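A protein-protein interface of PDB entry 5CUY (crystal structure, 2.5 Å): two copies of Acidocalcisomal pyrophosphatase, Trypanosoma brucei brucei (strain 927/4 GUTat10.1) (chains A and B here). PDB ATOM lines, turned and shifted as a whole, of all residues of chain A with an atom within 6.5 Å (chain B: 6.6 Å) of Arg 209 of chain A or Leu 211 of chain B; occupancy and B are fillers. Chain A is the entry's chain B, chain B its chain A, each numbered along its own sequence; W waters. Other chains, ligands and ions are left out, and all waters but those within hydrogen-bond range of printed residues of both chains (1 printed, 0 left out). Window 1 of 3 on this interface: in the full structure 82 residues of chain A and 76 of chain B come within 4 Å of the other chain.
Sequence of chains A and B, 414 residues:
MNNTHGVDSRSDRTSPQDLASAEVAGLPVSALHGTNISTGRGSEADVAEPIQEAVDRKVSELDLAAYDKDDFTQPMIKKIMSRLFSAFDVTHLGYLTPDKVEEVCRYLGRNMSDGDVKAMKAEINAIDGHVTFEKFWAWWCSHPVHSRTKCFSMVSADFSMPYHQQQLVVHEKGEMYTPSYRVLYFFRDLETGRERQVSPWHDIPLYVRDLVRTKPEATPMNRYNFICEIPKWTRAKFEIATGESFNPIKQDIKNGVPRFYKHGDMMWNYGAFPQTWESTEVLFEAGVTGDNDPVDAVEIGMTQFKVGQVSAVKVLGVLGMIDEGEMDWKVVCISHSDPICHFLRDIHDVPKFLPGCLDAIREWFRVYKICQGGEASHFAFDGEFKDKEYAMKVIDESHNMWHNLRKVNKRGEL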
ATOM      1  N   TYR A 163       0.755  10.613  -3.922  1.00  0.00           N
ATOM      2  CA  TYR A 163       0.892  11.175  -5.243  1.00  0.00           C
ATOM      3  C   TYR A 163       1.995  10.316  -5.849  1.00  0.00           C
ATOM      4  O   TYR A 163       2.640   9.544  -5.138  1.00  0.00           O
ATOM      5  CB  TYR A 163       1.289  12.665  -5.156  1.00  0.00           C
ATOM      6  CG  TYR A 163       2.660  12.948  -4.543  1.00  0.00           C
ATOM      7  CD1 TYR A 163       3.852  12.638  -5.228  1.00  0.00           C
ATOM      8  CD2 TYR A 163       2.769  13.504  -3.274  1.00  0.00           C
ATOM      9  CE1 TYR A 163       5.115  12.872  -4.658  1.00  0.00           C
ATOM     10  CE2 TYR A 163       4.027  13.742  -2.695  1.00  0.00           C
ATOM     11  CZ  TYR A 163       5.192  13.421  -3.388  1.00  0.00           C
ATOM     12  OH  TYR A 163       6.414  13.631  -2.778  1.00  0.00           O
ATOM     13  N   HIS A 164       2.191  10.407  -7.160  1.00  0.00           N
ATOM     14  CA  HIS A 164       3.248   9.643  -7.804  1.00  0.00           C
ATOM     15  C   HIS A 164       4.378  10.575  -8.188  1.00  0.00           C
ATOM     16  O   HIS A 164       4.166  11.635  -8.765  1.00  0.00           O
ATOM     17  CB  HIS A 164       2.756   8.946  -9.073  1.00  0.00           C
ATOM     18  CG  HIS A 164       1.430   8.267  -8.926  1.00  0.00           C
ATOM     19  ND1 HIS A 164       0.233   8.954  -8.960  1.00  0.00           N
ATOM     20  CD2 HIS A 164       1.112   6.958  -8.769  1.00  0.00           C
ATOM     21  CE1 HIS A 164      -0.767   8.098  -8.835  1.00  0.00           C
ATOM     22  NE2 HIS A 164      -0.261   6.881  -8.718  1.00  0.00           N
ATOM     23  N   GLN A 165       5.591  10.183  -7.854  1.00  0.00           N
ATOM     24  CA  GLN A 165       6.723  10.994  -8.234  1.00  0.00           C
ATOM     25  C   GLN A 165       6.828  10.984  -9.764  1.00  0.00           C
ATOM     26  O   GLN A 165       6.816   9.915 -10.389  1.00  0.00           O
ATOM     27  CB  GLN A 165       8.010  10.416  -7.640  1.00  0.00           C
ATOM     28  CG  GLN A 165       8.756  11.393  -6.760  1.00  0.00           C
ATOM     29  CD  GLN A 165      10.239  11.125  -6.718  1.00  0.00           C
ATOM     30  OE1 GLN A 165      10.690  10.048  -6.303  1.00  0.00           O
ATOM     31  NE2 GLN A 165      11.015  12.108  -7.154  1.00  0.00           N
ATOM     32  N   GLN A 166       6.905  12.164 -10.373  1.00  0.00           N
ATOM     33  CA  GLN A 166       7.078  12.230 -11.833  1.00  0.00           C
ATOM     34  C   GLN A 166       8.540  12.576 -12.108  1.00  0.00           C
ATOM     35  O   GLN A 166       9.095  13.508 -11.504  1.00  0.00           O
ATOM     36  CB  GLN A 166       6.206  13.325 -12.460  1.00  0.00           C
ATOM     37  CG  GLN A 166       4.712  13.141 -12.273  1.00  0.00           C
ATOM     38  CD  GLN A 166       4.187  11.929 -12.988  1.00  0.00           C
ATOM     39  OE1 GLN A 166       3.356  11.213 -12.465  1.00  0.00           O
ATOM     40  NE2 GLN A 166       4.665  11.692 -14.191  1.00  0.00           N
ATOM     41  N   GLN A 167       9.177  11.802 -12.978  1.00  0.00           N
ATOM     42  CA  GLN A 167      10.545  12.081 -13.367  1.00  0.00           C
ATOM     43  C   GLN A 167      10.512  12.750 -14.760  1.00  0.00           C
ATOM     44  O   GLN A 167       9.906  12.215 -15.702  1.00  0.00           O
ATOM     45  CB  GLN A 167      11.336  10.785 -13.426  1.00  0.00           C
ATOM     46  CG  GLN A 167      12.670  10.892 -14.155  1.00  0.00           C
ATOM     47  CD  GLN A 167      13.737  11.642 -13.371  1.00  0.00           C
ATOM     48  OE1 GLN A 167      14.125  11.215 -12.268  1.00  0.00           O
ATOM     49  NE2 GLN A 167      14.223  12.760 -13.931  1.00  0.00           N
ATOM     50  N   PHE A 187       6.991  12.966 -18.771  1.00  0.00           N
ATOM     51  CA  PHE A 187       6.920  12.648 -17.344  1.00  0.00           C
ATOM     52  C   PHE A 187       6.868  11.104 -17.272  1.00  0.00           C
ATOM     53  O   PHE A 187       6.156  10.429 -18.025  1.00  0.00           O
ATOM     54  CB  PHE A 187       5.656  13.194 -16.668  1.00  0.00           C
ATOM     55  CG  PHE A 187       5.786  14.574 -16.083  1.00  0.00           C
ATOM     56  CD1 PHE A 187       6.816  15.432 -16.451  1.00  0.00           C
ATOM     57  CD2 PHE A 187       4.775  15.066 -15.264  1.00  0.00           C
ATOM     58  CE1 PHE A 187       6.817  16.773 -16.024  1.00  0.00           C
ATOM     59  CE2 PHE A 187       4.762  16.392 -14.836  1.00  0.00           C
ATOM     60  CZ  PHE A 187       5.788  17.253 -15.223  1.00  0.00           C
ATOM     61  N   PRO A 205       6.667  22.576 -13.183  1.00  0.00           N
ATOM     62  CA  PRO A 205       6.304  23.531 -12.112  1.00  0.00           C
ATOM     63  C   PRO A 205       7.199  24.770 -12.079  1.00  0.00           C
ATOM     64  O   PRO A 205       8.406  24.644 -12.134  1.00  0.00           O
ATOM     65  CB  PRO A 205       6.460  22.709 -10.847  1.00  0.00           C
ATOM     66  CG  PRO A 205       6.352  21.287 -11.327  1.00  0.00           C
ATOM     67  CD  PRO A 205       7.047  21.271 -12.628  1.00  0.00           C
ATOM     68  N   TYR A 207       7.329  26.992  -9.498  1.00  0.00           N
ATOM     69  CA  TYR A 207       7.793  26.974  -8.118  1.00  0.00           C
ATOM     70  C   TYR A 207       8.077  25.491  -7.771  1.00  0.00           C
ATOM     71  O   TYR A 207       7.234  24.621  -7.977  1.00  0.00           O
ATOM     72  CB  TYR A 207       6.707  27.572  -7.190  1.00  0.00           C
ATOM     73  CG  TYR A 207       6.353  29.054  -7.411  1.00  0.00           C
ATOM     74  CD1 TYR A 207       7.158  30.060  -6.890  1.00  0.00           C
ATOM     75  CD2 TYR A 207       5.242  29.436  -8.155  1.00  0.00           C
ATOM     76  CE1 TYR A 207       6.887  31.407  -7.100  1.00  0.00           C
ATOM     77  CE2 TYR A 207       4.945  30.794  -8.383  1.00  0.00           C
ATOM     78  CZ  TYR A 207       5.787  31.766  -7.849  1.00  0.00           C
ATOM     79  OH  TYR A 207       5.590  33.114  -8.076  1.00  0.00           O
ATOM     80  N   VAL A 208       9.289  25.205  -7.305  1.00  0.00           N
ATOM     81  CA  VAL A 208       9.680  23.859  -6.923  1.00  0.00           C
ATOM     82  C   VAL A 208       9.371  23.771  -5.423  1.00  0.00           C
ATOM     83  O   VAL A 208      10.031  24.451  -4.621  1.00  0.00           O
ATOM     84  CB  VAL A 208      11.215  23.616  -7.120  1.00  0.00           C
ATOM     85  CG1 VAL A 208      11.588  22.223  -6.629  1.00  0.00           C
ATOM     86  CG2 VAL A 208      11.626  23.812  -8.580  1.00  0.00           C
ATOM     87  N   ARG A 209       8.397  22.946  -5.034  1.00  0.00           N
ATOM     88  CA  ARG A 209       8.022  22.845  -3.624  1.00  0.00           C
ATOM     89  C   ARG A 209       8.074  21.448  -3.031  1.00  0.00           C
ATOM     90  O   ARG A 209       7.675  20.476  -3.662  1.00  0.00           O
ATOM     91  CB  ARG A 209       6.637  23.444  -3.425  1.00  0.00           C
ATOM     92  CG  ARG A 209       6.636  24.950  -3.519  1.00  0.00           C
ATOM     93  CD  ARG A 209       5.236  25.484  -3.583  1.00  0.00           C
ATOM     94  NE  ARG A 209       5.160  26.951  -3.565  1.00  0.00           N
ATOM     95  CZ  ARG A 209       4.170  27.649  -4.148  1.00  0.00           C
ATOM     96  NH1 ARG A 209       3.173  27.020  -4.801  1.00  0.00           N
ATOM     97  NH2 ARG A 209       4.174  28.986  -4.082  1.00  0.00           N
ATOM     98  N   ASP A 210       8.600  21.352  -1.819  1.00  0.00           N
ATOM     99  CA  ASP A 210       8.695  20.072  -1.134  1.00  0.00           C
ATOM    100  C   ASP A 210       7.303  19.782  -0.612  1.00  0.00           C
ATOM    101  O   ASP A 210       6.659  20.704  -0.119  1.00  0.00           O
ATOM    102  CB  ASP A 210       9.638  20.208   0.037  1.00  0.00           C
ATOM    103  CG  ASP A 210      11.072  20.469  -0.393  1.00  0.00           C
ATOM    104  OD1 ASP A 210      11.699  19.518  -0.927  1.00  0.00           O
ATOM    105  OD2 ASP A 210      11.564  21.616  -0.188  1.00  0.00           O
ATOM    106  N   LEU A 211       6.800  18.553  -0.708  1.00  0.00           N
ATOM    107  CA  LEU A 211       5.460  18.379  -0.168  1.00  0.00           C
ATOM    108  C   LEU A 211       5.509  18.533   1.356  1.00  0.00           C
ATOM    109  O   LEU A 211       4.544  18.969   1.959  1.00  0.00           O
ATOM    110  CB  LEU A 211       4.832  17.050  -0.554  1.00  0.00           C
ATOM    111  CG  LEU A 211       3.315  17.256  -0.373  1.00  0.00           C
ATOM    112  CD1 LEU A 211       2.733  18.281  -1.396  1.00  0.00           C
ATOM    113  CD2 LEU A 211       2.640  15.932  -0.542  1.00  0.00           C
ATOM    114  N   VAL A 212       6.642  18.174   1.962  1.00  0.00           N
ATOM    115  CA  VAL A 212       6.880  18.374   3.397  1.00  0.00           C
ATOM    116  C   VAL A 212       8.192  19.184   3.494  1.00  0.00           C
ATOM    117  O   VAL A 212       9.318  18.650   3.445  1.00  0.00           O
ATOM    118  CB  VAL A 212       7.065  17.046   4.192  1.00  0.00           C
ATOM    119  CG1 VAL A 212       7.322  17.389   5.641  1.00  0.00           C
ATOM    120  CG2 VAL A 212       5.828  16.156   4.054  1.00  0.00           C
ATOM    121  N   MET A 221      11.237  30.786   0.728  1.00  0.00           N
ATOM    122  CA  MET A 221      11.288  29.848  -0.356  1.00  0.00           C
ATOM    123  C   MET A 221      11.833  30.586  -1.607  1.00  0.00           C
ATOM    124  O   MET A 221      11.397  31.704  -1.919  1.00  0.00           O
ATOM    125  CB  MET A 221       9.873  29.280  -0.628  1.00  0.00           C
ATOM    126  CG  MET A 221       9.212  28.525   0.562  1.00  0.00           C
ATOM    127  SD  MET A 221       7.633  27.516   0.221  1.00  0.00           S
ATOM    128  CE  MET A 221       8.293  26.135  -0.649  1.00  0.00           C
ATOM    129  N   ARG A 223      13.158  28.691  -5.077  1.00  0.00           N
ATOM    130  CA  ARG A 223      13.615  27.595  -5.892  1.00  0.00           C
ATOM    131  C   ARG A 223      12.693  27.492  -7.091  1.00  0.00           C
ATOM    132  O   ARG A 223      11.508  27.150  -6.973  1.00  0.00           O
ATOM    133  CB  ARG A 223      13.621  26.294  -5.084  1.00  0.00           C
ATOM    134  CG  ARG A 223      14.282  25.066  -5.801  1.00  0.00           C
ATOM    135  CD  ARG A 223      14.449  23.807  -4.915  1.00  0.00           C
ATOM    136  NE  ARG A 223      15.838  23.323  -4.917  1.00  0.00           N
ATOM    137  CZ  ARG A 223      16.778  23.732  -4.060  1.00  0.00           C
ATOM    138  NH1 ARG A 223      16.497  24.631  -3.119  1.00  0.00           N
ATOM    139  NH2 ARG A 223      18.006  23.247  -4.139  1.00  0.00           N
ATOM    140  N   MET B 161      -2.556  18.848  -8.209  1.00  0.00           N
ATOM    141  CA  MET B 161      -2.030  18.671  -6.848  1.00  0.00           C
ATOM    142  C   MET B 161      -3.088  19.091  -5.826  1.00  0.00           C
ATOM    143  O   MET B 161      -3.172  20.271  -5.434  1.00  0.00           O
ATOM    144  CB  MET B 161      -0.744  19.474  -6.599  1.00  0.00           C
ATOM    145  CG  MET B 161      -0.122  19.183  -5.211  1.00  0.00           C
ATOM    146  SD  MET B 161      -0.136  17.409  -4.573  1.00  0.00           S
ATOM    147  CE  MET B 161      -0.349  16.322  -6.110  1.00  0.00           C
ATOM    148  N   GLN B 165       0.924  21.948   0.592  1.00  0.00           N
ATOM    149  CA  GLN B 165       2.300  21.919   1.045  1.00  0.00           C
ATOM    150  C   GLN B 165       2.320  22.182   2.557  1.00  0.00           C
ATOM    151  O   GLN B 165       1.642  23.086   3.064  1.00  0.00           O
ATOM    152  CB  GLN B 165       3.101  22.992   0.310  1.00  0.00           C
ATOM    153  CG  GLN B 165       4.466  23.196   0.914  1.00  0.00           C
ATOM    154  CD  GLN B 165       5.346  24.125   0.116  1.00  0.00           C
ATOM    155  OE1 GLN B 165       4.875  25.151  -0.431  1.00  0.00           O
ATOM    156  NE2 GLN B 165       6.645  23.785   0.049  1.00  0.00           N
ATOM    157  N   GLU B 191      -1.109  26.878   3.053  1.00  0.00           N
ATOM    158  CA  GLU B 191      -2.239  27.563   2.452  1.00  0.00           C
ATOM    159  C   GLU B 191      -3.265  28.017   3.505  1.00  0.00           C
ATOM    160  O   GLU B 191      -3.770  29.139   3.461  1.00  0.00           O
ATOM    161  CB  GLU B 191      -2.906  26.662   1.426  1.00  0.00           C
ATOM    162  CG  GLU B 191      -2.176  26.624   0.090  1.00  0.00           C
ATOM    163  CD  GLU B 191      -3.016  25.976  -0.994  1.00  0.00           C
ATOM    164  OE1 GLU B 191      -4.275  26.111  -0.968  1.00  0.00           O
ATOM    165  OE2 GLU B 191      -2.411  25.343  -1.887  1.00  0.00           O
ATOM    166  N   ARG B 209      11.166  13.295  -1.695  1.00  0.00           N
ATOM    167  CA  ARG B 209      10.797  13.202  -3.120  1.00  0.00           C
ATOM    168  C   ARG B 209      10.316  14.549  -3.682  1.00  0.00           C
ATOM    169  O   ARG B 209       9.697  15.346  -2.981  1.00  0.00           O
ATOM    170  CB  ARG B 209       9.734  12.091  -3.332  1.00  0.00           C
ATOM    171  CG  ARG B 209      10.130  10.809  -2.590  1.00  0.00           C
ATOM    172  CD  ARG B 209       9.775   9.432  -3.228  1.00  0.00           C
ATOM    173  NE  ARG B 209      10.962   8.537  -3.341  1.00  0.00           N
ATOM    174  CZ  ARG B 209      10.994   7.226  -3.022  1.00  0.00           C
ATOM    175  NH1 ARG B 209       9.902   6.611  -2.546  1.00  0.00           N
ATOM    176  NH2 ARG B 209      12.115   6.507  -3.217  1.00  0.00           N
ATOM    177  N   ASP B 210      10.641  14.812  -4.940  1.00  0.00           N
ATOM    178  CA  ASP B 210      10.226  16.052  -5.607  1.00  0.00           C
ATOM    179  C   ASP B 210       8.902  15.707  -6.282  1.00  0.00           C
ATOM    180  O   ASP B 210       8.657  14.540  -6.592  1.00  0.00           O
ATOM    181  CB  ASP B 210      11.225  16.473  -6.728  1.00  0.00           C
ATOM    182  CG  ASP B 210      12.574  17.017  -6.199  1.00  0.00           C
ATOM    183  OD1 ASP B 210      12.586  18.148  -5.629  1.00  0.00           O
ATOM    184  OD2 ASP B 210      13.623  16.324  -6.375  1.00  0.00           O
ATOM    185  N   LEU B 211       8.049  16.699  -6.501  1.00  0.00           N
ATOM    186  CA  LEU B 211       6.801  16.441  -7.217  1.00  0.00           C
ATOM    187  C   LEU B 211       7.226  16.024  -8.639  1.00  0.00           C
ATOM    188  O   LEU B 211       6.859  14.944  -9.130  1.00  0.00           O
ATOM    189  CB  LEU B 211       5.925  17.697  -7.208  1.00  0.00           C
ATOM    190  CG  LEU B 211       5.369  17.912  -5.782  1.00  0.00           C
ATOM    191  CD1 LEU B 211       4.736  19.305  -5.600  1.00  0.00           C
ATOM    192  CD2 LEU B 211       4.322  16.821  -5.509  1.00  0.00           C
ATOM    193  N   VAL B 212       8.045  16.861  -9.267  1.00  0.00           N
ATOM    194  CA  VAL B 212       8.599  16.576 -10.582  1.00  0.00           C
ATOM    195  C   VAL B 212      10.130  16.593 -10.428  1.00  0.00           C
ATOM    196  O   VAL B 212      10.773  17.599 -10.060  1.00  0.00           O
ATOM    197  CB  VAL B 212       8.159  17.609 -11.648  1.00  0.00           C
ATOM    198  CG1 VAL B 212       8.606  17.181 -13.023  1.00  0.00           C
ATOM    199  CG2 VAL B 212       6.678  17.702 -11.657  1.00  0.00           C
ATOM    200  N   ARG B 213      10.730  15.441 -10.670  1.00  0.00           N
ATOM    201  CA  ARG B 213      12.165  15.373 -10.556  1.00  0.00           C
ATOM    202  C   ARG B 213      12.745  15.877 -11.865  1.00  0.00           C
ATOM    203  O   ARG B 213      12.430  15.370 -12.951  1.00  0.00           O
ATOM    204  CB  ARG B 213      12.577  13.937 -10.254  1.00  0.00           C
ATOM    205  CG  ARG B 213      14.048  13.719 -10.084  1.00  0.00           C
ATOM    206  CD  ARG B 213      14.234  12.402  -9.361  1.00  0.00           C
ATOM    207  NE  ARG B 213      15.608  12.269  -8.902  1.00  0.00           N
ATOM    208  CZ  ARG B 213      16.615  11.840  -9.653  1.00  0.00           C
ATOM    209  NH1 ARG B 213      16.418  11.477 -10.923  1.00  0.00           N
ATOM    210  NH2 ARG B 213      17.832  11.802  -9.130  1.00  0.00           N
HETATM  211  O   HOH W   1      12.649  13.475  -6.042  1.00  0.00           O
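Among the printed residues, pairs that only touch across the chains: Tyr 163 of chain A with Arg 209 of chain B, Gln 165 of chain A with Arg 213 of chain B, Gln 166 of chain A with Val 212 of chain B, Phe 187 of chain A with Val 212 of chain B, Pro 205 of chain A with Val 212 of chain B, Arg 209 of chain A with Gln 165 of chain B, Arg 209 of chain A with Leu 211 of chain B and Leu 211 of chain A with Gln 165 of chain B.
Gln 165 of chain A touches Arg 209 of chain B, and with the chains exchanged Arg 209 of chain A touches Gln 165 of chain B. Gln 165 of chain A touches Asp 210 of chain B, and with the chains exchanged Asp 210 of chain A touches Gln 165 of chain B. Arg 209 of chain A touches Leu 211 of chain B, but with the chains exchanged Leu 211 of chain A does not touch Arg 209 of chain B (4.9 Å). Leu 211 of chain A touches Gln 165 of chain B, but with the chains exchanged Gln 165 of chain A does not touch Leu 211 of chain B (4.01 Å). 5 positions are printed for both chains.
Of the printed residues of chain B, Tyr 163 of chain A touches Arg 209. His 164 of chain A touches none of the printed residues of chain B. Of the printed residues of chain B, Gln 167 of chain A touches Arg 213 (2.7 Å). Val 208 of chain A touches none of the printed residues of chain B. Arg 209 of chain A touches just these residues of chain B: Gln 165 and Leu 211. Printed residues of chain A within 4 Å of Leu 211 of chain B: Gln 166 (3.0 Å) and Arg 209 (3.7 Å). Printed residues of chain A within 4 Å of Val 212 of chain B: Gln 166, Phe 187 and Pro 205. The nearest printed residue of chain A that does not touch Gln 165 of chain B is Val 212 of chain A (5.6 Å).
Water W1 bridges NE2 of Gln 165 of chain A and N of Asp 210 of chain B.
Of the 8 printed residues of chain B, 6 touch a printed residue of chain A. Hydrophobic or aromatic side chains of chain B within 4 Å of the printed part of chain A: Leu 211 and Val 212. Along chain B the printed residues that touch a printed residue of chain A span positions 165 to 213. Of the 15 printed residues of chain A, 10 touch a printed residue of chain B. Hydrophobic or aromatic side chains of chain A within 4 Å of the printed part of chain B: Tyr 163, Phe 187, Pro 205 and Met 221. Along chain A the printed residues that touch a printed residue of chain B span positions 163 to 221.
The guanidinium group (NH1) of Arg 213 of chain B sits at hydrogen-bond distance from the side-chain amide oxygen (OE1) of Gln 167 of chain A (2.7 Å). NE2 of Gln 165 of chain B sits at hydrogen-bond distance from O of Asp 210 of chain A (3.1 Å). NE of Arg 209 of chain B lies close to OE1 of Gln 165 of chain A, 3.3 Å away. The side-chain sulfur (SD) of Met 221 of chain A sits close to the side-chain amide oxygen (OE1) of Gln 165 of chain B (3.7 Å). N of Gln 166 of chain A sits at hydrogen-bond distance from O of Leu 211 of chain B. N of Arg 213 of chain B sits at hydrogen-bond distance from O of Gln 166 of chain A, 2.7 Å away. The side-chain amide nitrogen of Gln 165 of chain A lies close to the backbone carbonyl oxygen of Asp 210 of chain B.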
